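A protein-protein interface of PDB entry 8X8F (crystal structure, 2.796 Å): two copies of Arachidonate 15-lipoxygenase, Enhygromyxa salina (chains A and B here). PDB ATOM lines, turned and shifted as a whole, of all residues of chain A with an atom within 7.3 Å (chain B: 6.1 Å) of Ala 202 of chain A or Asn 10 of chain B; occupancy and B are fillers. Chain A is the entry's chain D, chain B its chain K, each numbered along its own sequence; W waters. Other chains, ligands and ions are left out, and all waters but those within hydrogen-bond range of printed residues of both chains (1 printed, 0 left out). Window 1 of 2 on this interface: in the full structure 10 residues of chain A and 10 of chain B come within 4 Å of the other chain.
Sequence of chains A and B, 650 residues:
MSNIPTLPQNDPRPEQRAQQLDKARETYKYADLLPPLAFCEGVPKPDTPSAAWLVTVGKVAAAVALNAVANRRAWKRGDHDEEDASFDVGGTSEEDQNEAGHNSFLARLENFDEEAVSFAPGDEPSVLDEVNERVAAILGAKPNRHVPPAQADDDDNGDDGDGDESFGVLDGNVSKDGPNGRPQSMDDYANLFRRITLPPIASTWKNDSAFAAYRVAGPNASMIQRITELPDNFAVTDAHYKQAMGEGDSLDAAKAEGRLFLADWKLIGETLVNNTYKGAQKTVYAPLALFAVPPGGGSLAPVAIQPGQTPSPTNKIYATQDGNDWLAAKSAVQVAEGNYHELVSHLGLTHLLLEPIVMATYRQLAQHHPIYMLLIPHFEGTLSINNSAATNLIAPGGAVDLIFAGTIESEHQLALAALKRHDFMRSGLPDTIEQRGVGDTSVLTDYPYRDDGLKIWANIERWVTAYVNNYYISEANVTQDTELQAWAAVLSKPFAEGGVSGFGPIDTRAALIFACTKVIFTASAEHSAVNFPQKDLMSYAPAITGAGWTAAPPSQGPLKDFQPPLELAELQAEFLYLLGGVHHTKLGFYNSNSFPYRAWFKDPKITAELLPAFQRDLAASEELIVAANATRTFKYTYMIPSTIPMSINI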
ATOM      1  N   ALA A 190     -17.128  -7.061 -20.279  1.00  0.00           N
ATOM      2  CA  ALA A 190     -17.916  -5.998 -20.893  1.00  0.00           C
ATOM      3  C   ALA A 190     -17.084  -4.736 -21.079  1.00  0.00           C
ATOM      4  O   ALA A 190     -17.226  -4.035 -22.088  1.00  0.00           O
ATOM      5  CB  ALA A 190     -19.157  -5.707 -20.051  1.00  0.00           C
ATOM      6  N   PHE A 193     -15.338  -3.171 -24.421  1.00  0.00           N
ATOM      7  CA  PHE A 193     -16.018  -2.391 -25.451  1.00  0.00           C
ATOM      8  C   PHE A 193     -16.023  -0.924 -25.028  1.00  0.00           C
ATOM      9  O   PHE A 193     -17.013  -0.387 -24.523  1.00  0.00           O
ATOM     10  CB  PHE A 193     -17.430  -2.922 -25.671  1.00  0.00           C
ATOM     11  CG  PHE A 193     -17.482  -4.357 -26.124  1.00  0.00           C
ATOM     12  CD1 PHE A 193     -17.293  -5.395 -25.225  1.00  0.00           C
ATOM     13  CD2 PHE A 193     -17.743  -4.668 -27.447  1.00  0.00           C
ATOM     14  CE1 PHE A 193     -17.350  -6.712 -25.638  1.00  0.00           C
ATOM     15  CE2 PHE A 193     -17.802  -5.982 -27.866  1.00  0.00           C
ATOM     16  CZ  PHE A 193     -17.607  -7.005 -26.961  1.00  0.00           C
ATOM     17  N   LEU A 198     -21.081  -2.213 -26.702  1.00  0.00           N
ATOM     18  CA  LEU A 198     -21.388  -3.537 -26.176  1.00  0.00           C
ATOM     19  C   LEU A 198     -22.674  -4.067 -26.807  1.00  0.00           C
ATOM     20  O   LEU A 198     -23.689  -3.356 -26.824  1.00  0.00           O
ATOM     21  CB  LEU A 198     -21.528  -3.470 -24.655  1.00  0.00           C
ATOM     22  CG  LEU A 198     -21.721  -4.757 -23.850  1.00  0.00           C
ATOM     23  CD1 LEU A 198     -20.488  -5.636 -23.930  1.00  0.00           C
ATOM     24  CD2 LEU A 198     -22.039  -4.420 -22.403  1.00  0.00           C
ATOM     25  N   PRO A 199     -22.680  -5.299 -27.325  1.00  0.00           N
ATOM     26  CA  PRO A 199     -23.873  -5.795 -28.006  1.00  0.00           C
ATOM     27  C   PRO A 199     -24.995  -6.059 -27.020  1.00  0.00           C
ATOM     28  O   PRO A 199     -24.748  -6.308 -25.827  1.00  0.00           O
ATOM     29  CB  PRO A 199     -23.386  -7.098 -28.666  1.00  0.00           C
ATOM     30  CG  PRO A 199     -22.251  -7.539 -27.821  1.00  0.00           C
ATOM     31  CD  PRO A 199     -21.579  -6.277 -27.354  1.00  0.00           C
ATOM     32  N   PRO A 200     -26.253  -6.025 -27.474  1.00  0.00           N
ATOM     33  CA  PRO A 200     -27.378  -6.218 -26.543  1.00  0.00           C
ATOM     34  C   PRO A 200     -27.437  -7.608 -25.939  1.00  0.00           C
ATOM     35  O   PRO A 200     -28.082  -7.784 -24.899  1.00  0.00           O
ATOM     36  CB  PRO A 200     -28.613  -5.944 -27.416  1.00  0.00           C
ATOM     37  CG  PRO A 200     -28.091  -5.257 -28.648  1.00  0.00           C
ATOM     38  CD  PRO A 200     -26.714  -5.796 -28.853  1.00  0.00           C
ATOM     39  N   ILE A 201     -26.794  -8.601 -26.558  1.00  0.00           N
ATOM     40  CA  ILE A 201     -26.815  -9.952 -26.019  1.00  0.00           C
ATOM     41  C   ILE A 201     -26.009 -10.049 -24.729  1.00  0.00           C
ATOM     42  O   ILE A 201     -26.195 -10.992 -23.952  1.00  0.00           O
ATOM     43  CB  ILE A 201     -26.302 -10.944 -27.081  1.00  0.00           C
ATOM     44  CG1 ILE A 201     -26.505 -12.393 -26.630  1.00  0.00           C
ATOM     45  CG2 ILE A 201     -24.839 -10.675 -27.398  1.00  0.00           C
ATOM     46  CD1 ILE A 201     -27.935 -12.727 -26.278  1.00  0.00           C
ATOM     47  N   ALA A 202     -25.132  -9.076 -24.468  1.00  0.00           N
ATOM     48  CA  ALA A 202     -24.311  -9.113 -23.263  1.00  0.00           C
ATOM     49  C   ALA A 202     -25.140  -9.028 -21.991  1.00  0.00           C
ATOM     50  O   ALA A 202     -24.648  -9.391 -20.917  1.00  0.00           O
ATOM     51  CB  ALA A 202     -23.290  -7.977 -23.289  1.00  0.00           C
ATOM     52  N   SER A 203     -26.383  -8.565 -22.086  1.00  0.00           N
ATOM     53  CA  SER A 203     -27.239  -8.400 -20.924  1.00  0.00           C
ATOM     54  C   SER A 203     -28.416  -9.367 -20.904  1.00  0.00           C
ATOM     55  O   SER A 203     -29.251  -9.280 -20.000  1.00  0.00           O
ATOM     56  CB  SER A 203     -27.753  -6.958 -20.857  1.00  0.00           C
ATOM     57  OG  SER A 203     -26.709  -6.041 -21.135  1.00  0.00           O
ATOM     58  N   THR A 204     -28.519 -10.271 -21.879  1.00  0.00           N
ATOM     59  CA  THR A 204     -29.608 -11.238 -21.911  1.00  0.00           C
ATOM     60  C   THR A 204     -29.157 -12.657 -22.226  1.00  0.00           C
ATOM     61  O   THR A 204     -30.006 -13.551 -22.300  1.00  0.00           O
ATOM     62  CB  THR A 204     -30.674 -10.840 -22.947  1.00  0.00           C
ATOM     63  OG1 THR A 204     -30.142 -11.010 -24.267  1.00  0.00           O
ATOM     64  CG2 THR A 204     -31.117  -9.396 -22.760  1.00  0.00           C
ATOM     65  N   TRP A 205     -27.855 -12.891 -22.417  1.00  0.00           N
ATOM     66  CA  TRP A 205     -27.401 -14.187 -22.907  1.00  0.00           C
ATOM     67  C   TRP A 205     -27.655 -15.315 -21.917  1.00  0.00           C
ATOM     68  O   TRP A 205     -27.675 -16.482 -22.320  1.00  0.00           O
ATOM     69  CB  TRP A 205     -25.911 -14.129 -23.258  1.00  0.00           C
ATOM     70  CG  TRP A 205     -24.989 -14.088 -22.075  1.00  0.00           C
ATOM     71  CD1 TRP A 205     -24.490 -12.977 -21.462  1.00  0.00           C
ATOM     72  CD2 TRP A 205     -24.441 -15.212 -21.376  1.00  0.00           C
ATOM     73  NE1 TRP A 205     -23.670 -13.339 -20.419  1.00  0.00           N
ATOM     74  CE2 TRP A 205     -23.624 -14.706 -20.345  1.00  0.00           C
ATOM     75  CE3 TRP A 205     -24.565 -16.598 -21.519  1.00  0.00           C
ATOM     76  CZ2 TRP A 205     -22.934 -15.537 -19.463  1.00  0.00           C
ATOM     77  CZ3 TRP A 205     -23.881 -17.420 -20.642  1.00  0.00           C
ATOM     78  CH2 TRP A 205     -23.076 -16.889 -19.628  1.00  0.00           C
ATOM     79  N   LYS A 206     -27.848 -15.001 -20.638  1.00  0.00           N
ATOM     80  CA  LYS A 206     -28.115 -16.047 -19.662  1.00  0.00           C
ATOM     81  C   LYS A 206     -29.549 -16.551 -19.727  1.00  0.00           C
ATOM     82  O   LYS A 206     -29.816 -17.673 -19.286  1.00  0.00           O
ATOM     83  CB  LYS A 206     -27.811 -15.546 -18.252  1.00  0.00           C
ATOM     84  CG  LYS A 206     -26.446 -14.899 -18.098  1.00  0.00           C
ATOM     85  CD  LYS A 206     -26.012 -14.923 -16.643  1.00  0.00           C
ATOM     86  CE  LYS A 206     -24.794 -14.044 -16.403  1.00  0.00           C
ATOM     87  NZ  LYS A 206     -24.357 -14.055 -14.975  1.00  0.00           N
ATOM     88  N   ASN A 207     -30.469 -15.749 -20.266  1.00  0.00           N
ATOM     89  CA  ASN A 207     -31.865 -16.152 -20.356  1.00  0.00           C
ATOM     90  C   ASN A 207     -32.017 -17.385 -21.235  1.00  0.00           C
ATOM     91  O   ASN A 207     -31.337 -17.531 -22.253  1.00  0.00           O
ATOM     92  CB  ASN A 207     -32.711 -15.010 -20.919  1.00  0.00           C
ATOM     93  CG  ASN A 207     -33.117 -14.005 -19.861  1.00  0.00           C
ATOM     94  OD1 ASN A 207     -33.597 -14.374 -18.790  1.00  0.00           O
ATOM     95  ND2 ASN A 207     -32.923 -12.725 -20.156  1.00  0.00           N
ATOM     96  N   ASP A 536     -23.020  -8.676 -33.801  1.00  0.00           N
ATOM     97  CA  ASP A 536     -24.106  -8.457 -32.854  1.00  0.00           C
ATOM     98  C   ASP A 536     -24.198  -9.541 -31.789  1.00  0.00           C
ATOM     99  O   ASP A 536     -24.552  -9.247 -30.644  1.00  0.00           O
ATOM    100  CB  ASP A 536     -25.437  -8.362 -33.603  1.00  0.00           C
ATOM    101  CG  ASP A 536     -25.451  -7.245 -34.627  1.00  0.00           C
ATOM    102  OD1 ASP A 536     -24.697  -6.268 -34.447  1.00  0.00           O
ATOM    103  OD2 ASP A 536     -26.215  -7.344 -35.610  1.00  0.00           O
ATOM    104  N   LEU A 537     -23.898 -10.795 -32.131  1.00  0.00           N
ATOM    105  CA  LEU A 537     -24.152 -11.901 -31.220  1.00  0.00           C
ATOM    106  C   LEU A 537     -22.902 -12.627 -30.752  1.00  0.00           C
ATOM    107  O   LEU A 537     -22.958 -13.317 -29.730  1.00  0.00           O
ATOM    108  CB  LEU A 537     -25.095 -12.920 -31.878  1.00  0.00           C
ATOM    109  CG  LEU A 537     -26.444 -12.372 -32.350  1.00  0.00           C
ATOM    110  CD1 LEU A 537     -27.236 -13.427 -33.112  1.00  0.00           C
ATOM    111  CD2 LEU A 537     -27.249 -11.836 -31.175  1.00  0.00           C
ATOM    112  N   TYR A 540     -19.138 -10.844 -27.869  1.00  0.00           N
ATOM    113  CA  TYR A 540     -19.046 -10.856 -26.411  1.00  0.00           C
ATOM    114  C   TYR A 540     -18.795 -12.293 -25.969  1.00  0.00           C
ATOM    115  O   TYR A 540     -19.680 -13.147 -26.091  1.00  0.00           O
ATOM    116  CB  TYR A 540     -20.320 -10.286 -25.791  1.00  0.00           C
ATOM    117  CG  TYR A 540     -20.339 -10.244 -24.279  1.00  0.00           C
ATOM    118  CD1 TYR A 540     -19.451  -9.442 -23.572  1.00  0.00           C
ATOM    119  CD2 TYR A 540     -21.265 -10.988 -23.561  1.00  0.00           C
ATOM    120  CE1 TYR A 540     -19.476  -9.398 -22.186  1.00  0.00           C
ATOM    121  CE2 TYR A 540     -21.299 -10.948 -22.180  1.00  0.00           C
ATOM    122  CZ  TYR A 540     -20.404 -10.152 -21.498  1.00  0.00           C
ATOM    123  OH  TYR A 540     -20.443 -10.118 -20.123  1.00  0.00           O
ATOM    124  N   PRO A 542     -18.559 -14.156 -23.132  1.00  0.00           N
ATOM    125  CA  PRO A 542     -19.442 -14.960 -22.268  1.00  0.00           C
ATOM    126  C   PRO A 542     -20.720 -15.410 -22.953  1.00  0.00           C
ATOM    127  O   PRO A 542     -21.279 -16.448 -22.577  1.00  0.00           O
ATOM    128  CB  PRO A 542     -19.732 -14.020 -21.090  1.00  0.00           C
ATOM    129  CG  PRO A 542     -18.572 -13.100 -21.055  1.00  0.00           C
ATOM    130  CD  PRO A 542     -18.204 -12.875 -22.492  1.00  0.00           C
ATOM    131  N   ALA A 543     -21.200 -14.663 -23.951  1.00  0.00           N
ATOM    132  CA  ALA A 543     -22.398 -15.080 -24.671  1.00  0.00           C
ATOM    133  C   ALA A 543     -22.121 -16.290 -25.553  1.00  0.00           C
ATOM    134  O   ALA A 543     -22.953 -17.200 -25.643  1.00  0.00           O
ATOM    135  CB  ALA A 543     -22.939 -13.916 -25.504  1.00  0.00           C
ATOM    136  N   THR B   6     -31.069  -3.637 -15.889  1.00  0.00           N
ATOM    137  CA  THR B   6     -30.846  -5.072 -15.950  1.00  0.00           C
ATOM    138  C   THR B   6     -31.284  -5.724 -14.649  1.00  0.00           C
ATOM    139  O   THR B   6     -31.160  -5.139 -13.569  1.00  0.00           O
ATOM    140  CB  THR B   6     -29.371  -5.420 -16.187  1.00  0.00           C
ATOM    141  OG1 THR B   6     -28.627  -4.226 -16.459  1.00  0.00           O
ATOM    142  CG2 THR B   6     -29.229  -6.389 -17.346  1.00  0.00           C
ATOM    143  N   LEU B   7     -31.797  -6.942 -14.762  1.00  0.00           N
ATOM    144  CA  LEU B   7     -31.876  -7.800 -13.599  1.00  0.00           C
ATOM    145  C   LEU B   7     -30.457  -8.149 -13.148  1.00  0.00           C
ATOM    146  O   LEU B   7     -29.535  -8.189 -13.969  1.00  0.00           O
ATOM    147  CB  LEU B   7     -32.665  -9.067 -13.917  1.00  0.00           C
ATOM    148  CG  LEU B   7     -34.145  -8.863 -14.252  1.00  0.00           C
ATOM    149  CD1 LEU B   7     -34.876 -10.194 -14.274  1.00  0.00           C
ATOM    150  CD2 LEU B   7     -34.806  -7.900 -13.271  1.00  0.00           C
ATOM    151  N   PRO B   8     -30.245  -8.380 -11.848  1.00  0.00           N
ATOM    152  CA  PRO B   8     -28.863  -8.547 -11.368  1.00  0.00           C
ATOM    153  C   PRO B   8     -28.173  -9.790 -11.903  1.00  0.00           C
ATOM    154  O   PRO B   8     -26.946  -9.777 -12.060  1.00  0.00           O
ATOM    155  CB  PRO B   8     -29.026  -8.598  -9.843  1.00  0.00           C
ATOM    156  CG  PRO B   8     -30.398  -9.102  -9.638  1.00  0.00           C
ATOM    157  CD  PRO B   8     -31.224  -8.528 -10.757  1.00  0.00           C
ATOM    158  N   GLN B   9     -28.910 -10.860 -12.195  1.00  0.00           N
ATOM    159  CA  GLN B   9     -28.289 -12.054 -12.755  1.00  0.00           C
ATOM    160  C   GLN B   9     -28.022 -11.936 -14.247  1.00  0.00           C
ATOM    161  O   GLN B   9     -27.476 -12.874 -14.835  1.00  0.00           O
ATOM    162  CB  GLN B   9     -29.154 -13.290 -12.480  1.00  0.00           C
ATOM    163  CG  GLN B   9     -30.493 -13.314 -13.204  1.00  0.00           C
ATOM    164  CD  GLN B   9     -31.617 -12.702 -12.388  1.00  0.00           C
ATOM    165  OE1 GLN B   9     -31.390 -11.839 -11.541  1.00  0.00           O
ATOM    166  NE2 GLN B   9     -32.841 -13.157 -12.637  1.00  0.00           N
ATOM    167  N   ASN B  10     -28.387 -10.819 -14.871  1.00  0.00           N
ATOM    168  CA  ASN B  10     -28.105 -10.576 -16.279  1.00  0.00           C
ATOM    169  C   ASN B  10     -27.173  -9.393 -16.494  1.00  0.00           C
ATOM    170  O   ASN B  10     -26.793  -9.117 -17.636  1.00  0.00           O
ATOM    171  CB  ASN B  10     -29.415 -10.347 -17.045  1.00  0.00           C
ATOM    172  CG  ASN B  10     -30.222 -11.621 -17.222  1.00  0.00           C
ATOM    173  OD1 ASN B  10     -29.686 -12.725 -17.135  1.00  0.00           O
ATOM    174  ND2 ASN B  10     -31.517 -11.470 -17.484  1.00  0.00           N
ATOM    175  N   ASP B  11     -26.798  -8.695 -15.426  1.00  0.00           N
ATOM    176  CA  ASP B  11     -26.016  -7.476 -15.557  1.00  0.00           C
ATOM    177  C   ASP B  11     -24.619  -7.813 -16.067  1.00  0.00           C
ATOM    178  O   ASP B  11     -23.947  -8.679 -15.492  1.00  0.00           O
ATOM    179  CB  ASP B  11     -25.941  -6.755 -14.209  1.00  0.00           C
ATOM    180  CG  ASP B  11     -25.675  -5.266 -14.345  1.00  0.00           C
ATOM    181  OD1 ASP B  11     -26.545  -4.541 -14.872  1.00  0.00           O
ATOM    182  OD2 ASP B  11     -24.598  -4.817 -13.908  1.00  0.00           O
ATOM    183  N   PRO B  12     -24.155  -7.175 -17.145  1.00  0.00           N
ATOM    184  CA  PRO B  12     -22.829  -7.505 -17.685  1.00  0.00           C
ATOM    185  C   PRO B  12     -21.676  -7.015 -16.827  1.00  0.00           C
ATOM    186  O   PRO B  12     -20.525  -7.358 -17.125  1.00  0.00           O
ATOM    187  CB  PRO B  12     -22.831  -6.817 -19.054  1.00  0.00           C
ATOM    188  CG  PRO B  12     -23.744  -5.655 -18.873  1.00  0.00           C
ATOM    189  CD  PRO B  12     -24.820  -6.115 -17.920  1.00  0.00           C
ATOM    190  N   ARG B  13     -21.933  -6.227 -15.785  1.00  0.00           N
ATOM    191  CA  ARG B  13     -20.883  -5.743 -14.887  1.00  0.00           C
ATOM    192  C   ARG B  13     -21.347  -5.910 -13.446  1.00  0.00           C
ATOM    193  O   ARG B  13     -21.669  -4.934 -12.760  1.00  0.00           O
ATOM    194  CB  ARG B  13     -20.533  -4.285 -15.195  1.00  0.00           C
ATOM    195  CG  ARG B  13     -19.997  -4.049 -16.597  1.00  0.00           C
ATOM    196  CD  ARG B  13     -20.784  -2.960 -17.308  1.00  0.00           C
ATOM    197  NE  ARG B  13     -20.232  -2.654 -18.625  1.00  0.00           N
ATOM    198  CZ  ARG B  13     -19.302  -1.731 -18.843  1.00  0.00           C
ATOM    199  NH1 ARG B  13     -18.818  -1.024 -17.831  1.00  0.00           N
ATOM    200  NH2 ARG B  13     -18.856  -1.517 -20.073  1.00  0.00           N
ATOM    201  N   ASN B 477     -37.011 -15.530 -13.648  1.00  0.00           N
ATOM    202  CA  ASN B 477     -36.351 -14.262 -13.351  1.00  0.00           C
ATOM    203  C   ASN B 477     -36.619 -13.823 -11.917  1.00  0.00           C
ATOM    204  O   ASN B 477     -35.727 -13.293 -11.245  1.00  0.00           O
ATOM    205  CB  ASN B 477     -36.813 -13.180 -14.328  1.00  0.00           C
ATOM    206  CG  ASN B 477     -36.280 -13.389 -15.734  1.00  0.00           C
ATOM    207  OD1 ASN B 477     -36.939 -13.044 -16.717  1.00  0.00           O
ATOM    208  ND2 ASN B 477     -35.084 -13.954 -15.838  1.00  0.00           N
HETATM  209  O   HOH W   1     -32.096 -14.781 -15.857  1.00  0.00           O
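The side-chain amide nitrogen (ND2) of Asn 10 of chain B lies close to the side-chain amide nitrogen (ND2) of Asn 207 of chain A (3.3 Å).
O of Gln 9 of chain B sits close to NZ of Lys 206 of chain A.
The backbone carbonyl oxygen (O) of Ser 203 of chain A sits close to the backbone carbonyl oxygen (O) of Asn 10 of chain B (3.4 Å).
The side-chain amide oxygen of Asn 207 of chain A sits at hydrogen-bond distance from the side-chain amide nitrogen of Asn 477 of chain B (3.3 Å).
OD1 of Asp 11 of chain B sits at hydrogen-bond distance from OG1 of Thr 6 of chain B, at 2.6 Å.
The backbone carbonyl oxygen (O) of Asn 477 of chain B lies within hydrogen-bond range of the side-chain amide nitrogen (NE2) of Gln 9 of chain B (3.2 Å).
Among the printed residues, pairs that only touch across the chains: Ala 190 of chain A with Arg 13 of chain B, Lys 206 of chain A with Asn 10 of chain B, Ala 190 of chain A with Pro 12 of chain B, Ala 202 of chain A with Pro 12 of chain B, Ser 203 of chain A with Pro 12 of chain B, Ser 203 of chain A with Thr 6 of chain B and Ala 202 of chain A with Asn 10 of chain B.
Of the printed residues of chain B, Ala 190 of chain A touches Pro 12 (3.6 Å) and Arg 13 (3.5 Å).
Of chain B, only Asn 10 (3.9 Å) and Pro 12 (3.7 Å) come within 4 Å of Ala 202 of chain A.
Of the printed residues of chain B, Asn 207 of chain A touches Asn 10 (3.3 Å) and Asn 477 (3.3 Å).
Printed residues of chain A within 4 Å of Thr 6 of chain B: Ser 203 (3.9 Å).
Pro 8 of chain B touches none of the printed residues of chain A.
Of the printed residues of chain A, Gln 9 of chain B touches Lys 206.
Asn 10 of chain B touches four residues of chain A.
Printed residues of chain A within 4 Å of Pro 12 of chain B: Ala 190, Ala 202 and Ser 203.
The nearest residue of chain A that does not touch Asn 10 of chain B is Thr 204 of chain A (4.7 Å).
Of the 9 printed residues of chain B, 6 touch a printed residue of chain A.
Hydrophobic or aromatic side chains of chain B within 4 Å of the printed part of chain A: Pro 12.
Among the printed residues, no Asp or Glu carboxylate lies within 4 Å of a Lys or Arg side-chain nitrogen of the other chain.
No position is printed for both chains.
Water W1 lies within hydrogen-bond range of the side-chain amide nitrogen (ND2) of Asn 477 of chain B (3.1 Å), the side-chain amide oxygen (OD1) of Asn 207 of chain A (3.3 Å) and the side-chain amide oxygen (OD1) of Asn 10 of chain B (3.4 Å).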
